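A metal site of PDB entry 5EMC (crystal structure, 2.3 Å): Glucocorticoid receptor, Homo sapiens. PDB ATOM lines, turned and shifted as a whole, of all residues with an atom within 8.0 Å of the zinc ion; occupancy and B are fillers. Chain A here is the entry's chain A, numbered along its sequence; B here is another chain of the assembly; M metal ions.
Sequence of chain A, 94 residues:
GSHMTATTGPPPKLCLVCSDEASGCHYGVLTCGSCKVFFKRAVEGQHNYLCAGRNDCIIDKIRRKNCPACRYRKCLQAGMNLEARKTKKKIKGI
The side-chain sulfur (SG) of Cys 15 sits close to the backbone NH (N) of Val 17 (3.4 Å).
The backbone NH (N) of Cys 15 is in hydrogen-bond range of the backbone carbonyl oxygen (O) of Asp 20 (2.7 Å).
The guanidinium group of Arg 64 sits close to the side-chain sulfur of Cys 18, 3.3 Å away.
SG of Cys 18 lies close to N of Asp 20, at 3.4 Å.
The backbone carbonyl oxygen of Cys 18 is in hydrogen-bond range of the backbone NH of Lys 61.
SG of Cys 35 sits close to NH2 of Arg 71 (3.7 Å).
The side-chain sulfur (SG) of Cys 32 sits close to the side-chain hydroxyl (OG) of Ser 34 (3.0 Å).
Four residues have an atom within 4 Å of the zinc ion: Cys 15, Cys 18, Cys 32 and Cys 35.
The nearest printed residue that does not touch the zinc ion is Val 17 (4.4 Å).
SG of Cys 15 binds the zinc ion.
The zinc ion is bound by SG of Cys 18 (2.3 Å).
The zinc ion is bound by SG of Cys 35, 2.4 Å away.
SG of Cys 32 is bound to the zinc ion.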
ATOM      1  N   LEU A  14     -10.020  -4.800   7.094  1.00  0.00           N
ATOM      2  CA  LEU A  14      -9.370  -5.344   8.282  1.00  0.00           C
ATOM      3  C   LEU A  14      -7.853  -5.167   8.259  1.00  0.00           C
ATOM      4  O   LEU A  14      -7.181  -5.525   7.292  1.00  0.00           O
ATOM      5  CB  LEU A  14      -9.701  -6.834   8.445  1.00  0.00           C
ATOM      6  CG  LEU A  14     -11.144  -7.145   8.859  1.00  0.00           C
ATOM      7  CD1 LEU A  14     -11.319  -8.621   9.164  1.00  0.00           C
ATOM      8  CD2 LEU A  14     -11.550  -6.290  10.055  1.00  0.00           C
ATOM      9  N   CYS A  15      -7.337  -4.613   9.350  1.00  0.00           N
ATOM     10  CA  CYS A  15      -5.909  -4.499   9.573  1.00  0.00           C
ATOM     11  C   CYS A  15      -5.208  -5.835   9.317  1.00  0.00           C
ATOM     12  O   CYS A  15      -5.619  -6.866   9.838  1.00  0.00           O
ATOM     13  CB  CYS A  15      -5.630  -4.036  11.006  1.00  0.00           C
ATOM     14  SG  CYS A  15      -3.886  -3.841  11.413  1.00  0.00           S
ATOM     15  N   LEU A  16      -4.169  -5.811   8.496  1.00  0.00           N
ATOM     16  CA  LEU A  16      -3.460  -7.035   8.126  1.00  0.00           C
ATOM     17  C   LEU A  16      -2.652  -7.557   9.300  1.00  0.00           C
ATOM     18  O   LEU A  16      -2.304  -8.736   9.354  1.00  0.00           O
ATOM     19  CB  LEU A  16      -2.551  -6.800   6.924  1.00  0.00           C
ATOM     20  N   VAL A  17      -2.371  -6.673  10.252  1.00  0.00           N
ATOM     21  CA  VAL A  17      -1.540  -7.034  11.390  1.00  0.00           C
ATOM     22  C   VAL A  17      -2.388  -7.601  12.520  1.00  0.00           C
ATOM     23  O   VAL A  17      -2.111  -8.695  13.012  1.00  0.00           O
ATOM     24  CB  VAL A  17      -0.722  -5.822  11.866  1.00  0.00           C
ATOM     25  CG1 VAL A  17       0.165  -6.204  13.042  1.00  0.00           C
ATOM     26  CG2 VAL A  17       0.127  -5.290  10.713  1.00  0.00           C
ATOM     27  N   CYS A  18      -3.434  -6.881  12.934  1.00  0.00           N
ATOM     28  CA  CYS A  18      -4.199  -7.317  14.094  1.00  0.00           C
ATOM     29  C   CYS A  18      -5.665  -7.656  13.815  1.00  0.00           C
ATOM     30  O   CYS A  18      -6.390  -8.078  14.711  1.00  0.00           O
ATOM     31  CB  CYS A  18      -4.140  -6.249  15.189  1.00  0.00           C
ATOM     32  SG  CYS A  18      -5.129  -4.777  14.850  1.00  0.00           S
ATOM     33  N   SER A  19      -6.099  -7.462  12.571  1.00  0.00           N
ATOM     34  CA  SER A  19      -7.473  -7.769  12.141  1.00  0.00           C
ATOM     35  C   SER A  19      -8.515  -6.870  12.812  1.00  0.00           C
ATOM     36  O   SER A  19      -9.727  -7.116  12.708  1.00  0.00           O
ATOM     37  CB  SER A  19      -7.803  -9.243  12.415  1.00  0.00           C
ATOM     38  OG  SER A  19      -6.849 -10.092  11.803  1.00  0.00           O
ATOM     39  N   ASP A  20      -8.055  -5.827  13.495  1.00  0.00           N
ATOM     40  CA  ASP A  20      -8.951  -4.755  13.884  1.00  0.00           C
ATOM     41  C   ASP A  20      -9.364  -3.988  12.628  1.00  0.00           C
ATOM     42  O   ASP A  20      -8.732  -4.109  11.573  1.00  0.00           O
ATOM     43  CB  ASP A  20      -8.293  -3.821  14.896  1.00  0.00           C
ATOM     44  CG  ASP A  20      -9.272  -2.869  15.544  1.00  0.00           C
ATOM     45  OD1 ASP A  20     -10.492  -3.112  15.463  1.00  0.00           O
ATOM     46  OD2 ASP A  20      -8.816  -1.874  16.148  1.00  0.00           O
ATOM     47  N   GLU A  21     -10.437  -3.206  12.748  1.00  0.00           N
ATOM     48  CA  GLU A  21     -10.918  -2.387  11.646  1.00  0.00           C
ATOM     49  C   GLU A  21      -9.841  -1.387  11.194  1.00  0.00           C
ATOM     50  O   GLU A  21      -9.440  -0.489  11.954  1.00  0.00           O
ATOM     51  CB  GLU A  21     -12.178  -1.644  12.053  1.00  0.00           C
ATOM     52  CG  GLU A  21     -12.648  -0.630  11.033  1.00  0.00           C
ATOM     53  CD  GLU A  21     -14.148  -0.574  10.926  1.00  0.00           C
ATOM     54  OE1 GLU A  21     -14.824  -0.822  11.944  1.00  0.00           O
ATOM     55  OE2 GLU A  21     -14.656  -0.300   9.812  1.00  0.00           O
ATOM     56  N   ALA A  22      -9.375  -1.555   9.966  1.00  0.00           N
ATOM     57  CA  ALA A  22      -8.362  -0.682   9.376  1.00  0.00           C
ATOM     58  C   ALA A  22      -8.920   0.707   9.132  1.00  0.00           C
ATOM     59  O   ALA A  22     -10.138   0.911   9.130  1.00  0.00           O
ATOM     60  CB  ALA A  22      -7.837  -1.276   8.078  1.00  0.00           C
ATOM     61  N   LEU A  30      -2.579  -1.917   4.335  1.00  0.00           N
ATOM     62  CA  LEU A  30      -3.817  -1.647   5.033  1.00  0.00           C
ATOM     63  C   LEU A  30      -3.674  -2.045   6.506  1.00  0.00           C
ATOM     64  O   LEU A  30      -3.578  -3.241   6.832  1.00  0.00           O
ATOM     65  CB  LEU A  30      -4.976  -2.397   4.380  1.00  0.00           C
ATOM     66  CG  LEU A  30      -6.373  -2.100   4.940  1.00  0.00           C
ATOM     67  CD1 LEU A  30      -6.745  -0.648   4.691  1.00  0.00           C
ATOM     68  CD2 LEU A  30      -7.400  -3.029   4.339  1.00  0.00           C
ATOM     69  N   THR A  31      -3.620  -1.058   7.395  1.00  0.00           N
ATOM     70  CA  THR A  31      -3.532  -1.312   8.837  1.00  0.00           C
ATOM     71  C   THR A  31      -4.457  -0.374   9.600  1.00  0.00           C
ATOM     72  O   THR A  31      -5.021   0.552   9.030  1.00  0.00           O
ATOM     73  CB  THR A  31      -2.095  -1.126   9.389  1.00  0.00           C
ATOM     74  OG1 THR A  31      -1.765   0.270   9.418  1.00  0.00           O
ATOM     75  CG2 THR A  31      -1.071  -1.882   8.565  1.00  0.00           C
ATOM     76  N   CYS A  32      -4.588  -0.606  10.909  1.00  0.00           N
ATOM     77  CA  CYS A  32      -5.356   0.277  11.770  1.00  0.00           C
ATOM     78  C   CYS A  32      -4.480   1.430  12.273  1.00  0.00           C
ATOM     79  O   CYS A  32      -3.269   1.468  12.015  1.00  0.00           O
ATOM     80  CB  CYS A  32      -5.949  -0.503  12.947  1.00  0.00           C
ATOM     81  SG  CYS A  32      -4.736  -1.162  14.117  1.00  0.00           S
ATOM     82  N   GLY A  33      -5.086   2.366  12.992  1.00  0.00           N
ATOM     83  CA  GLY A  33      -4.347   3.505  13.519  1.00  0.00           C
ATOM     84  C   GLY A  33      -3.316   3.145  14.555  1.00  0.00           C
ATOM     85  O   GLY A  33      -2.200   3.649  14.532  1.00  0.00           O
ATOM     86  N   SER A  34      -3.695   2.248  15.475  1.00  0.00           N
ATOM     87  CA  SER A  34      -2.787   1.830  16.541  1.00  0.00           C
ATOM     88  C   SER A  34      -1.549   1.139  15.973  1.00  0.00           C
ATOM     89  O   SER A  34      -0.436   1.366  16.444  1.00  0.00           O
ATOM     90  CB  SER A  34      -3.510   0.924  17.536  1.00  0.00           C
ATOM     91  OG  SER A  34      -4.070  -0.210  16.891  1.00  0.00           O
ATOM     92  N   CYS A  35      -1.761   0.302  14.952  1.00  0.00           N
ATOM     93  CA  CYS A  35      -0.652  -0.391  14.306  1.00  0.00           C
ATOM     94  C   CYS A  35       0.252   0.544  13.507  1.00  0.00           C
ATOM     95  O   CYS A  35       1.461   0.345  13.428  1.00  0.00           O
ATOM     96  CB  CYS A  35      -1.183  -1.498  13.390  1.00  0.00           C
ATOM     97  SG  CYS A  35      -1.562  -3.030  14.287  1.00  0.00           S
ATOM     98  N   LYS A  36      -0.353   1.569  12.921  1.00  0.00           N
ATOM     99  CA  LYS A  36       0.402   2.562  12.182  1.00  0.00           C
ATOM    100  C   LYS A  36       1.403   3.239  13.098  1.00  0.00           C
ATOM    101  O   LYS A  36       2.600   3.285  12.812  1.00  0.00           O
ATOM    102  CB  LYS A  36      -0.542   3.595  11.549  1.00  0.00           C
ATOM    103  CG  LYS A  36       0.141   4.882  11.126  1.00  0.00           C
ATOM    104  CD  LYS A  36      -0.860   5.892  10.589  1.00  0.00           C
ATOM    105  CE  LYS A  36      -0.234   7.261  10.453  1.00  0.00           C
ATOM    106  NZ  LYS A  36      -0.052   7.910  11.788  1.00  0.00           N
ATOM    107  N   PHE A  38       2.288   2.329  16.159  1.00  0.00           N
ATOM    108  CA  PHE A  38       3.185   1.368  16.789  1.00  0.00           C
ATOM    109  C   PHE A  38       4.376   1.128  15.863  1.00  0.00           C
ATOM    110  O   PHE A  38       5.530   1.187  16.307  1.00  0.00           O
ATOM    111  CB  PHE A  38       2.481   0.037  17.085  1.00  0.00           C
ATOM    112  CG  PHE A  38       3.423  -1.070  17.462  1.00  0.00           C
ATOM    113  CD1 PHE A  38       3.861  -1.981  16.509  1.00  0.00           C
ATOM    114  CD2 PHE A  38       3.897  -1.184  18.758  1.00  0.00           C
ATOM    115  CE1 PHE A  38       4.750  -2.986  16.851  1.00  0.00           C
ATOM    116  CE2 PHE A  38       4.767  -2.191  19.103  1.00  0.00           C
ATOM    117  CZ  PHE A  38       5.203  -3.099  18.140  1.00  0.00           C
ATOM    118  N   ILE A  59      -1.576 -12.211  17.238  1.00  0.00           N
ATOM    119  CA  ILE A  59      -1.735 -10.768  17.275  1.00  0.00           C
ATOM    120  C   ILE A  59      -3.125 -10.384  16.760  1.00  0.00           C
ATOM    121  O   ILE A  59      -3.361 -10.342  15.557  1.00  0.00           O
ATOM    122  CB  ILE A  59      -0.654 -10.055  16.445  1.00  0.00           C
ATOM    123  CG1 ILE A  59       0.734 -10.541  16.853  1.00  0.00           C
ATOM    124  CG2 ILE A  59      -0.740  -8.551  16.629  1.00  0.00           C
ATOM    125  CD1 ILE A  59       1.154 -10.123  18.252  1.00  0.00           C
ATOM    126  N   ASP A  60      -4.046 -10.121  17.689  1.00  0.00           N
ATOM    127  CA  ASP A  60      -5.340  -9.595  17.334  1.00  0.00           C
ATOM    128  C   ASP A  60      -5.577  -8.300  18.106  1.00  0.00           C
ATOM    129  O   ASP A  60      -4.656  -7.811  18.782  1.00  0.00           O
ATOM    130  CB  ASP A  60      -6.457 -10.609  17.596  1.00  0.00           C
ATOM    131  CG  ASP A  60      -6.478 -11.132  19.041  1.00  0.00           C
ATOM    132  OD1 ASP A  60      -6.156 -10.382  19.988  1.00  0.00           O
ATOM    133  OD2 ASP A  60      -6.843 -12.314  19.222  1.00  0.00           O
ATOM    134  N   LYS A  61      -6.792  -7.756  18.032  1.00  0.00           N
ATOM    135  CA  LYS A  61      -7.135  -6.471  18.657  1.00  0.00           C
ATOM    136  C   LYS A  61      -6.719  -6.402  20.125  1.00  0.00           C
ATOM    137  O   LYS A  61      -6.332  -5.338  20.602  1.00  0.00           O
ATOM    138  CB  LYS A  61      -8.644  -6.203  18.545  1.00  0.00           C
ATOM    139  N   ARG A  64      -2.343  -7.887  20.593  1.00  0.00           N
ATOM    140  CA  ARG A  64      -1.276  -7.105  19.967  1.00  0.00           C
ATOM    141  C   ARG A  64      -0.461  -6.337  21.000  1.00  0.00           C
ATOM    142  O   ARG A  64       0.726  -6.076  20.795  1.00  0.00           O
ATOM    143  CB  ARG A  64      -1.865  -6.148  18.912  1.00  0.00           C
ATOM    144  CG  ARG A  64      -2.476  -4.886  19.471  1.00  0.00           C
ATOM    145  CD  ARG A  64      -3.434  -4.256  18.489  1.00  0.00           C
ATOM    146  NE  ARG A  64      -4.047  -3.064  19.069  1.00  0.00           N
ATOM    147  CZ  ARG A  64      -5.170  -2.515  18.634  1.00  0.00           C
ATOM    148  NH1 ARG A  64      -5.661  -1.436  19.225  1.00  0.00           N
ATOM    149  NH2 ARG A  64      -5.805  -3.038  17.591  1.00  0.00           N
ATOM    150  N   ARG A  71       4.540  -8.333  17.272  1.00  0.00           N
ATOM    151  CA  ARG A  71       3.726  -7.366  16.569  1.00  0.00           C
ATOM    152  C   ARG A  71       4.549  -6.645  15.512  1.00  0.00           C
ATOM    153  O   ARG A  71       4.098  -6.468  14.381  1.00  0.00           O
ATOM    154  CB  ARG A  71       3.123  -6.367  17.551  1.00  0.00           C
ATOM    155  CG  ARG A  71       2.155  -5.390  16.925  1.00  0.00           C
ATOM    156  CD  ARG A  71       1.719  -4.373  17.975  1.00  0.00           C
ATOM    157  NE  ARG A  71       0.663  -3.488  17.490  1.00  0.00           N
ATOM    158  CZ  ARG A  71       0.082  -2.572  18.242  1.00  0.00           C
ATOM    159  NH1 ARG A  71       0.460  -2.428  19.506  1.00  0.00           N
ATOM    160  NH2 ARG A  71      -0.875  -1.805  17.748  1.00  0.00           N
ATOM    161  N   CYS A  75       4.266  -6.880  11.338  1.00  0.00           N
ATOM    162  CA  CYS A  75       4.228  -5.673  10.532  1.00  0.00           C
ATOM    163  C   CYS A  75       5.170  -5.809   9.345  1.00  0.00           C
ATOM    164  O   CYS A  75       4.800  -5.539   8.200  1.00  0.00           O
ATOM    165  CB  CYS A  75       4.617  -4.438  11.359  1.00  0.00           C
ATOM    166  SG  CYS A  75       3.368  -3.811  12.512  1.00  0.00           S
ATOM    167  N   MET A  80       5.147  -3.475   5.657  1.00  0.00           N
ATOM    168  CA  MET A  80       5.170  -2.093   6.105  1.00  0.00           C
ATOM    169  C   MET A  80       6.582  -1.528   6.072  1.00  0.00           C
ATOM    170  O   MET A  80       7.539  -2.222   6.440  1.00  0.00           O
ATOM    171  CB  MET A  80       4.586  -1.969   7.515  1.00  0.00           C
ATOM    172  CG  MET A  80       3.158  -2.451   7.650  1.00  0.00           C
ATOM    173  SD  MET A  80       2.526  -2.241   9.337  1.00  0.00           S
ATOM    174  CE  MET A  80       2.518  -0.455   9.442  1.00  0.00           C
ATOM    175  P    DG B  13      -2.651  -0.667  21.135  1.00  0.00           P
ATOM    176  OP1  DG B  13      -3.511  -1.860  21.306  1.00  0.00           O
ATOM    177  OP2  DG B  13      -1.689  -0.592  20.012  1.00  0.00           O
ATOM    178  O5'  DG B  13      -3.606   0.609  21.047  1.00  0.00           O
ATOM    179  C5'  DG B  13      -4.491   0.871  22.118  1.00  0.00           C
ATOM    180  C4'  DG B  13      -5.168   2.211  21.938  1.00  0.00           C
ATOM    181  O4'  DG B  13      -4.262   3.281  22.283  1.00  0.00           O
ATOM    182  C3'  DG B  13      -5.661   2.511  20.524  1.00  0.00           C
ATOM    183  O3'  DG B  13      -6.951   3.065  20.600  1.00  0.00           O
ATOM    184  C2'  DG B  13      -4.652   3.536  20.015  1.00  0.00           C
ATOM    185  C1'  DG B  13      -4.354   4.283  21.292  1.00  0.00           C
ATOM    186  N9   DG B  13      -3.096   5.015  21.269  1.00  0.00           N
ATOM    187  C8   DG B  13      -1.862   4.546  20.921  1.00  0.00           C
ATOM    188  N7   DG B  13      -0.919   5.446  21.016  1.00  0.00           N
ATOM    189  C5   DG B  13      -1.593   6.588  21.450  1.00  0.00           C
ATOM    190  C6   DG B  13      -1.106   7.868  21.728  1.00  0.00           C
ATOM    191  O6   DG B  13       0.061   8.281  21.638  1.00  0.00           O
ATOM    192  N1   DG B  13      -2.110   8.722  22.157  1.00  0.00           N
ATOM    193  C2   DG B  13      -3.431   8.375  22.279  1.00  0.00           C
ATOM    194  N2   DG B  13      -4.273   9.325  22.696  1.00  0.00           N
ATOM    195  N3   DG B  13      -3.902   7.172  22.024  1.00  0.00           N
ATOM    196  C4   DG B  13      -2.927   6.332  21.613  1.00  0.00           C
HETATM  197 ZN    ZN M   1      -3.821  -3.289  13.644  1.00  0.00          ZN
